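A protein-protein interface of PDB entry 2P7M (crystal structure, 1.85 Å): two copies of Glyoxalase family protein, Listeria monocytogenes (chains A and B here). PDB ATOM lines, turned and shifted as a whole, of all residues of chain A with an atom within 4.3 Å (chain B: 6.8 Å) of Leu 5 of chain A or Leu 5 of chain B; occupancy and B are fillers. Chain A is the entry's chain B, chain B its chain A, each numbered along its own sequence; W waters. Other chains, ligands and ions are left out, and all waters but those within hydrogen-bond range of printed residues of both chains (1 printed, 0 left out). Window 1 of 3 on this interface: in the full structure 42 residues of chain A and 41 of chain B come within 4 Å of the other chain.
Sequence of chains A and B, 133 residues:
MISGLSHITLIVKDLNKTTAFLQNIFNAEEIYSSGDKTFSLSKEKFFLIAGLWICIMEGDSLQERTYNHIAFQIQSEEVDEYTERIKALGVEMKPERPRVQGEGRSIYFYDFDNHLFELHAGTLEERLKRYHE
Of the 7 printed residues of chain A, 7 touch a printed residue of chain B.
Among the printed residues, 18 pairs touch across the chains.
A ring nitrogen (ND1) of His 7 of chain B is in hydrogen-bond range of the side-chain hydroxyl (OG) of Ser 6 of chain B.
OG of Ser 6 of chain A is in hydrogen-bond range of ND1 of His 7 of chain A (2.8 Å).
Leu 5 of chain A touches its own counterpart, Leu 5 of chain B.
Leu 5 of chain A touches Leu 52 of chain B, and with the chains exchanged Leu 52 of chain A touches Leu 5 of chain B.
Leu 5 of chain A touches Ile 70 of chain B, and with the chains exchanged Ile 70 of chain A touches Leu 5 of chain B.
Ser 6 of chain A touches Ala 71 of chain B, and with the chains exchanged Ala 71 of chain A touches Ser 6 of chain B.
Positions printed for both chains: 4, 5, 6, 7, 52, 70 and 71.
Of the 18 pairs that touch across the chains among the printed residues, 13 have their exchanged pair printed and touching as well.
Water W1 lies within hydrogen-bond range of OE1 of Gln 73 of chain B (2.6 Å) and OG of Ser 6 of chain A (2.8 Å).
O of Ala 71 of chain A sits at hydrogen-bond distance from N of Ser 6 of chain B (2.7 Å).
N of Ala 71 of chain A sits at hydrogen-bond distance from O of His 7 of chain B (2.9 Å).
The backbone NH (N) of Ser 6 of chain A sits at hydrogen-bond distance from the backbone carbonyl oxygen (O) of Ala 71 of chain B, at 2.7 Å.
N of Ala 71 of chain B sits at hydrogen-bond distance from O of His 7 of chain A.
The backbone NH (N) of Gln 73 of chain B is in hydrogen-bond range of the backbone carbonyl oxygen (O) of Gly 4 of chain A (2.7 Å).
Of chain B, only Leu 5, Leu 52, Ile 70 and Ala 71 come within 4 Å of Leu 5 of chain A.
Of chain A, only Leu 5, Leu 52, Ile 70 and Ala 71 come within 4 Å of Leu 5 of chain B.
Printed residues of chain A within 4 Å of Ser 6 of chain B: Ala 71 (2.7 Å).
Printed residues of chain B within 4 Å of Leu 52 of chain A: Leu 5.
Of the printed residues of chain A, Ala 71 of chain B touches Leu 5 (3.5 Å), Ser 6 (2.7 Å) and His 7 (2.9 Å).
Of the printed residues of chain A, Leu 52 of chain B touches Leu 5.
The nearest residue of chain B that does not touch Leu 5 of chain A is Gln 73 of chain B (4.3 Å).
The nearest printed residue of chain A that does not touch Leu 5 of chain B is His 7 of chain A (8.1 Å).
Among the printed residues, pairs that only touch across the chains: Gly 4 of chain A with Ala 50 of chain B (3.5 Å), Gly 4 of chain A with Phe 72 of chain B (3.4 Å), Leu 5 of chain A with Leu 5 of chain B (3.9 Å), Leu 5 of chain A with Leu 52 of chain B (3.5 Å), Leu 5 of chain A with Ile 70 of chain B (3.8 Å), Leu 5 of chain A with Ala 71 of chain B (3.5 Å), Ser 6 of chain A with Phe 72 of chain B (3.8 Å), Ser 6 of chain A with Gln 73 of chain B (3.8 Å), His 7 of chain A with Ile 70 of chain B (3.9 Å), Leu 52 of chain A with Leu 5 of chain B (3.6 Å), Ile 70 of chain A with Leu 5 of chain B (3.9 Å), Ile 70 of chain A with His 7 of chain B (3.9 Å) and Ala 71 of chain A with Leu 5 of chain B (3.5 Å).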
ATOM      1  N   GLY A   4      -5.852   7.255   2.699  1.00  0.00           N
ATOM      2  CA  GLY A   4      -5.483   8.430   3.473  1.00  0.00           C
ATOM      3  C   GLY A   4      -4.107   8.967   3.114  1.00  0.00           C
ATOM      4  O   GLY A   4      -3.567   8.657   2.053  1.00  0.00           O
ATOM      5  N   LEU A   5      -3.536   9.772   4.005  1.00  0.00           N
ATOM      6  CA  LEU A   5      -2.216  10.359   3.787  1.00  0.00           C
ATOM      7  C   LEU A   5      -1.104   9.371   4.116  1.00  0.00           C
ATOM      8  O   LEU A   5      -1.137   8.718   5.160  1.00  0.00           O
ATOM      9  CB  LEU A   5      -2.045  11.607   4.663  1.00  0.00           C
ATOM     10  CG  LEU A   5      -0.686  12.322   4.612  1.00  0.00           C
ATOM     11  CD1 LEU A   5      -0.531  13.035   3.285  1.00  0.00           C
ATOM     12  CD2 LEU A   5      -0.587  13.326   5.751  1.00  0.00           C
ATOM     13  N   SER A   6      -0.127   9.247   3.227  1.00  0.00           N
ATOM     14  CA  SER A   6       1.005   8.363   3.487  1.00  0.00           C
ATOM     15  C   SER A   6       2.099   9.187   4.158  1.00  0.00           C
ATOM     16  O   SER A   6       2.535   8.864   5.259  1.00  0.00           O
ATOM     17  CB  SER A   6       1.546   7.751   2.200  1.00  0.00           C
ATOM     18  OG  SER A   6       2.737   7.028   2.472  1.00  0.00           O
ATOM     19  N   HIS A   7       2.523  10.264   3.500  1.00  0.00           N
ATOM     20  CA  HIS A   7       3.560  11.133   4.053  1.00  0.00           C
ATOM     21  C   HIS A   7       3.704  12.423   3.261  1.00  0.00           C
ATOM     22  O   HIS A   7       3.089  12.576   2.218  1.00  0.00           O
ATOM     23  CB  HIS A   7       4.916  10.418   4.071  1.00  0.00           C
ATOM     24  CG  HIS A   7       5.367   9.919   2.734  1.00  0.00           C
ATOM     25  ND1 HIS A   7       4.956   8.711   2.212  1.00  0.00           N
ATOM     26  CD2 HIS A   7       6.214  10.453   1.820  1.00  0.00           C
ATOM     27  CE1 HIS A   7       5.533   8.520   1.039  1.00  0.00           C
ATOM     28  NE2 HIS A   7       6.302   9.563   0.778  1.00  0.00           N
ATOM     29  N   LEU A  52       2.065  12.223  11.875  1.00  0.00           N
ATOM     30  CA  LEU A  52       2.269  12.333  10.434  1.00  0.00           C
ATOM     31  C   LEU A  52       3.709  12.050  10.038  1.00  0.00           C
ATOM     32  O   LEU A  52       4.649  12.569  10.645  1.00  0.00           O
ATOM     33  CB  LEU A  52       1.894  13.728   9.955  1.00  0.00           C
ATOM     34  CG  LEU A  52       0.520  14.237  10.380  1.00  0.00           C
ATOM     35  CD1 LEU A  52       0.418  15.719  10.050  1.00  0.00           C
ATOM     36  CD2 LEU A  52      -0.576  13.436   9.682  1.00  0.00           C
ATOM     37  N   ILE A  70       1.476  24.031   3.668  1.00  0.00           N
ATOM     38  CA  ILE A  70       0.942  23.033   4.577  1.00  0.00           C
ATOM     39  C   ILE A  70       0.476  23.754   5.839  1.00  0.00           C
ATOM     40  O   ILE A  70       1.144  24.670   6.325  1.00  0.00           O
ATOM     41  CB  ILE A  70       2.039  22.023   4.968  1.00  0.00           C
ATOM     42  CG1 ILE A  70       2.615  21.376   3.711  1.00  0.00           C
ATOM     43  CG2 ILE A  70       1.477  20.980   5.928  1.00  0.00           C
ATOM     44  CD1 ILE A  70       3.907  20.640   3.944  1.00  0.00           C
ATOM     45  N   ALA A  71      -0.665  23.334   6.375  1.00  0.00           N
ATOM     46  CA  ALA A  71      -1.204  23.946   7.582  1.00  0.00           C
ATOM     47  C   ALA A  71      -1.415  22.912   8.675  1.00  0.00           C
ATOM     48  O   ALA A  71      -2.151  21.935   8.485  1.00  0.00           O
ATOM     49  CB  ALA A  71      -2.525  24.650   7.276  1.00  0.00           C
ATOM     50  N   ILE B   2       1.565  20.199  18.284  1.00  0.00           N
ATOM     51  CA  ILE B   2       0.729  20.228  17.095  1.00  0.00           C
ATOM     52  C   ILE B   2      -0.351  19.160  17.226  1.00  0.00           C
ATOM     53  O   ILE B   2      -0.045  18.007  17.521  1.00  0.00           O
ATOM     54  CB  ILE B   2       1.564  19.944  15.838  1.00  0.00           C
ATOM     55  CG1 ILE B   2       2.697  20.970  15.725  1.00  0.00           C
ATOM     56  CG2 ILE B   2       0.675  19.962  14.605  1.00  0.00           C
ATOM     57  CD1 ILE B   2       2.224  22.408  15.689  1.00  0.00           C
ATOM     58  N   SER B   3      -1.606  19.549  17.013  1.00  0.00           N
ATOM     59  CA  SER B   3      -2.738  18.624  17.104  1.00  0.00           C
ATOM     60  C   SER B   3      -2.701  17.650  15.939  1.00  0.00           C
ATOM     61  O   SER B   3      -3.059  16.481  16.070  1.00  0.00           O
ATOM     62  CB  SER B   3      -4.060  19.393  17.065  1.00  0.00           C
ATOM     63  OG  SER B   3      -4.098  20.399  18.062  1.00  0.00           O
ATOM     64  N   GLY B   4      -2.266  18.150  14.789  1.00  0.00           N
ATOM     65  CA  GLY B   4      -2.186  17.321  13.606  1.00  0.00           C
ATOM     66  C   GLY B   4      -2.258  18.168  12.354  1.00  0.00           C
ATOM     67  O   GLY B   4      -2.003  19.375  12.385  1.00  0.00           O
ATOM     68  N   LEU B   5      -2.611  17.534  11.246  1.00  0.00           N
ATOM     69  CA  LEU B   5      -2.720  18.239   9.979  1.00  0.00           C
ATOM     70  C   LEU B   5      -4.043  18.993   9.909  1.00  0.00           C
ATOM     71  O   LEU B   5      -5.096  18.445  10.229  1.00  0.00           O
ATOM     72  CB  LEU B   5      -2.630  17.238   8.828  1.00  0.00           C
ATOM     73  CG  LEU B   5      -2.597  17.801   7.410  1.00  0.00           C
ATOM     74  CD1 LEU B   5      -1.380  18.711   7.241  1.00  0.00           C
ATOM     75  CD2 LEU B   5      -2.552  16.645   6.421  1.00  0.00           C
ATOM     76  N   SER B   6      -3.995  20.260   9.513  1.00  0.00           N
ATOM     77  CA  SER B   6      -5.224  21.029   9.386  1.00  0.00           C
ATOM     78  C   SER B   6      -5.716  20.888   7.947  1.00  0.00           C
ATOM     79  O   SER B   6      -6.827  20.414   7.698  1.00  0.00           O
ATOM     80  CB  SER B   6      -4.988  22.506   9.704  1.00  0.00           C
ATOM     81  OG  SER B   6      -6.182  23.244   9.493  1.00  0.00           O
ATOM     82  N   HIS B   7      -4.873  21.299   7.005  1.00  0.00           N
ATOM     83  CA  HIS B   7      -5.203  21.218   5.590  1.00  0.00           C
ATOM     84  C   HIS B   7      -4.004  21.568   4.722  1.00  0.00           C
ATOM     85  O   HIS B   7      -2.976  22.038   5.217  1.00  0.00           O
ATOM     86  CB  HIS B   7      -6.356  22.165   5.254  1.00  0.00           C
ATOM     87  CG  HIS B   7      -6.063  23.601   5.556  1.00  0.00           C
ATOM     88  ND1 HIS B   7      -6.238  24.149   6.805  1.00  0.00           N
ATOM     89  CD2 HIS B   7      -5.585  24.597   4.772  1.00  0.00           C
ATOM     90  CE1 HIS B   7      -5.883  25.422   6.781  1.00  0.00           C
ATOM     91  NE2 HIS B   7      -5.482  25.718   5.559  1.00  0.00           N
ATOM     92  N   ILE B   8      -4.154  21.333   3.421  1.00  0.00           N
ATOM     93  CA  ILE B   8      -3.115  21.617   2.445  1.00  0.00           C
ATOM     94  C   ILE B   8      -3.694  22.603   1.429  1.00  0.00           C
ATOM     95  O   ILE B   8      -4.813  22.423   0.950  1.00  0.00           O
ATOM     96  CB  ILE B   8      -2.679  20.320   1.728  1.00  0.00           C
ATOM     97  CG1 ILE B   8      -2.141  19.322   2.760  1.00  0.00           C
ATOM     98  CG2 ILE B   8      -1.629  20.629   0.681  1.00  0.00           C
ATOM     99  CD1 ILE B   8      -1.844  17.952   2.196  1.00  0.00           C
ATOM    100  N   ILE B  49     -10.418  14.724   0.704  1.00  0.00           N
ATOM    101  CA  ILE B  49      -9.791  13.618  -0.013  1.00  0.00           C
ATOM    102  C   ILE B  49      -9.201  12.648   0.994  1.00  0.00           C
ATOM    103  O   ILE B  49      -8.186  12.938   1.621  1.00  0.00           O
ATOM    104  CB  ILE B  49      -8.649  14.101  -0.932  1.00  0.00           C
ATOM    105  CG1 ILE B  49      -9.190  15.031  -2.015  1.00  0.00           C
ATOM    106  CG2 ILE B  49      -7.956  12.908  -1.562  1.00  0.00           C
ATOM    107  CD1 ILE B  49      -8.118  15.551  -2.954  1.00  0.00           C
ATOM    108  N   ALA B  50      -9.849  11.499   1.153  1.00  0.00           N
ATOM    109  CA  ALA B  50      -9.389  10.481   2.090  1.00  0.00           C
ATOM    110  C   ALA B  50      -9.165  11.060   3.481  1.00  0.00           C
ATOM    111  O   ALA B  50      -8.109  10.864   4.087  1.00  0.00           O
ATOM    112  CB  ALA B  50      -8.101   9.834   1.573  1.00  0.00           C
ATOM    113  N   LEU B  52      -8.559  14.002   4.331  1.00  0.00           N
ATOM    114  CA  LEU B  52      -7.728  15.198   4.344  1.00  0.00           C
ATOM    115  C   LEU B  52      -8.441  16.380   3.708  1.00  0.00           C
ATOM    116  O   LEU B  52      -9.093  16.236   2.676  1.00  0.00           O
ATOM    117  CB  LEU B  52      -6.428  14.941   3.582  1.00  0.00           C
ATOM    118  CG  LEU B  52      -5.635  13.694   3.973  1.00  0.00           C
ATOM    119  CD1 LEU B  52      -4.422  13.570   3.060  1.00  0.00           C
ATOM    120  CD2 LEU B  52      -5.205  13.782   5.438  1.00  0.00           C
ATOM    121  N   TRP B  53      -8.318  17.551   4.324  1.00  0.00           N
ATOM    122  CA  TRP B  53      -8.929  18.753   3.774  1.00  0.00           C
ATOM    123  C   TRP B  53      -7.943  19.377   2.804  1.00  0.00           C
ATOM    124  O   TRP B  53      -6.801  19.646   3.161  1.00  0.00           O
ATOM    125  CB  TRP B  53      -9.262  19.756   4.880  1.00  0.00           C
ATOM    126  CG  TRP B  53     -10.454  19.375   5.685  1.00  0.00           C
ATOM    127  CD1 TRP B  53     -10.589  18.277   6.480  1.00  0.00           C
ATOM    128  CD2 TRP B  53     -11.694  20.088   5.768  1.00  0.00           C
ATOM    129  NE1 TRP B  53     -11.839  18.258   7.056  1.00  0.00           N
ATOM    130  CE2 TRP B  53     -12.537  19.359   6.636  1.00  0.00           C
ATOM    131  CE3 TRP B  53     -12.177  21.272   5.194  1.00  0.00           C
ATOM    132  CZ2 TRP B  53     -13.836  19.775   6.947  1.00  0.00           C
ATOM    133  CZ3 TRP B  53     -13.471  21.688   5.504  1.00  0.00           C
ATOM    134  CH2 TRP B  53     -14.284  20.938   6.373  1.00  0.00           C
ATOM    135  N   ILE B  70       3.167  15.704  -1.838  1.00  0.00           N
ATOM    136  CA  ILE B  70       2.287  14.990  -0.926  1.00  0.00           C
ATOM    137  C   ILE B  70       2.085  13.570  -1.424  1.00  0.00           C
ATOM    138  O   ILE B  70       1.891  13.341  -2.615  1.00  0.00           O
ATOM    139  CB  ILE B  70       0.920  15.691  -0.837  1.00  0.00           C
ATOM    140  CG1 ILE B  70       1.100  17.076  -0.219  1.00  0.00           C
ATOM    141  CG2 ILE B  70      -0.041  14.868   0.002  1.00  0.00           C
ATOM    142  CD1 ILE B  70      -0.030  18.013  -0.525  1.00  0.00           C
ATOM    143  N   ALA B  71       2.135  12.605  -0.519  1.00  0.00           N
ATOM    144  CA  ALA B  71       1.945  11.229  -0.934  1.00  0.00           C
ATOM    145  C   ALA B  71       0.740  10.611  -0.232  1.00  0.00           C
ATOM    146  O   ALA B  71       0.636  10.641   0.996  1.00  0.00           O
ATOM    147  CB  ALA B  71       3.210  10.417  -0.654  1.00  0.00           C
ATOM    148  N   PHE B  72      -0.181  10.065  -1.023  1.00  0.00           N
ATOM    149  CA  PHE B  72      -1.369   9.432  -0.468  1.00  0.00           C
ATOM    150  C   PHE B  72      -1.169   7.931  -0.409  1.00  0.00           C
ATOM    151  O   PHE B  72      -0.351   7.370  -1.141  1.00  0.00           O
ATOM    152  CB  PHE B  72      -2.604   9.736  -1.319  1.00  0.00           C
ATOM    153  CG  PHE B  72      -2.989  11.176  -1.331  1.00  0.00           C
ATOM    154  CD1 PHE B  72      -2.483  12.037  -2.301  1.00  0.00           C
ATOM    155  CD2 PHE B  72      -3.849  11.685  -0.363  1.00  0.00           C
ATOM    156  CE1 PHE B  72      -2.830  13.384  -2.306  1.00  0.00           C
ATOM    157  CE2 PHE B  72      -4.202  13.033  -0.359  1.00  0.00           C
ATOM    158  CZ  PHE B  72      -3.689  13.883  -1.333  1.00  0.00           C
ATOM    159  N   GLN B  73      -1.931   7.278   0.456  1.00  0.00           N
ATOM    160  CA  GLN B  73      -1.823   5.840   0.609  1.00  0.00           C
ATOM    161  C   GLN B  73      -2.830   5.074  -0.224  1.00  0.00           C
ATOM    162  O   GLN B  73      -4.010   5.412  -0.245  1.00  0.00           O
ATOM    163  CB  GLN B  73      -2.027   5.452   2.075  1.00  0.00           C
ATOM    164  CG  GLN B  73      -1.923   3.955   2.331  1.00  0.00           C
ATOM    165  CD  GLN B  73      -0.509   3.519   2.652  1.00  0.00           C
ATOM    166  OE1 GLN B  73       0.081   3.994   3.620  1.00  0.00           O
ATOM    167  NE2 GLN B  73       0.042   2.611   1.845  1.00  0.00           N
HETATM  168  O   HOH W   1       2.582   4.693   3.968  1.00  0.00           O
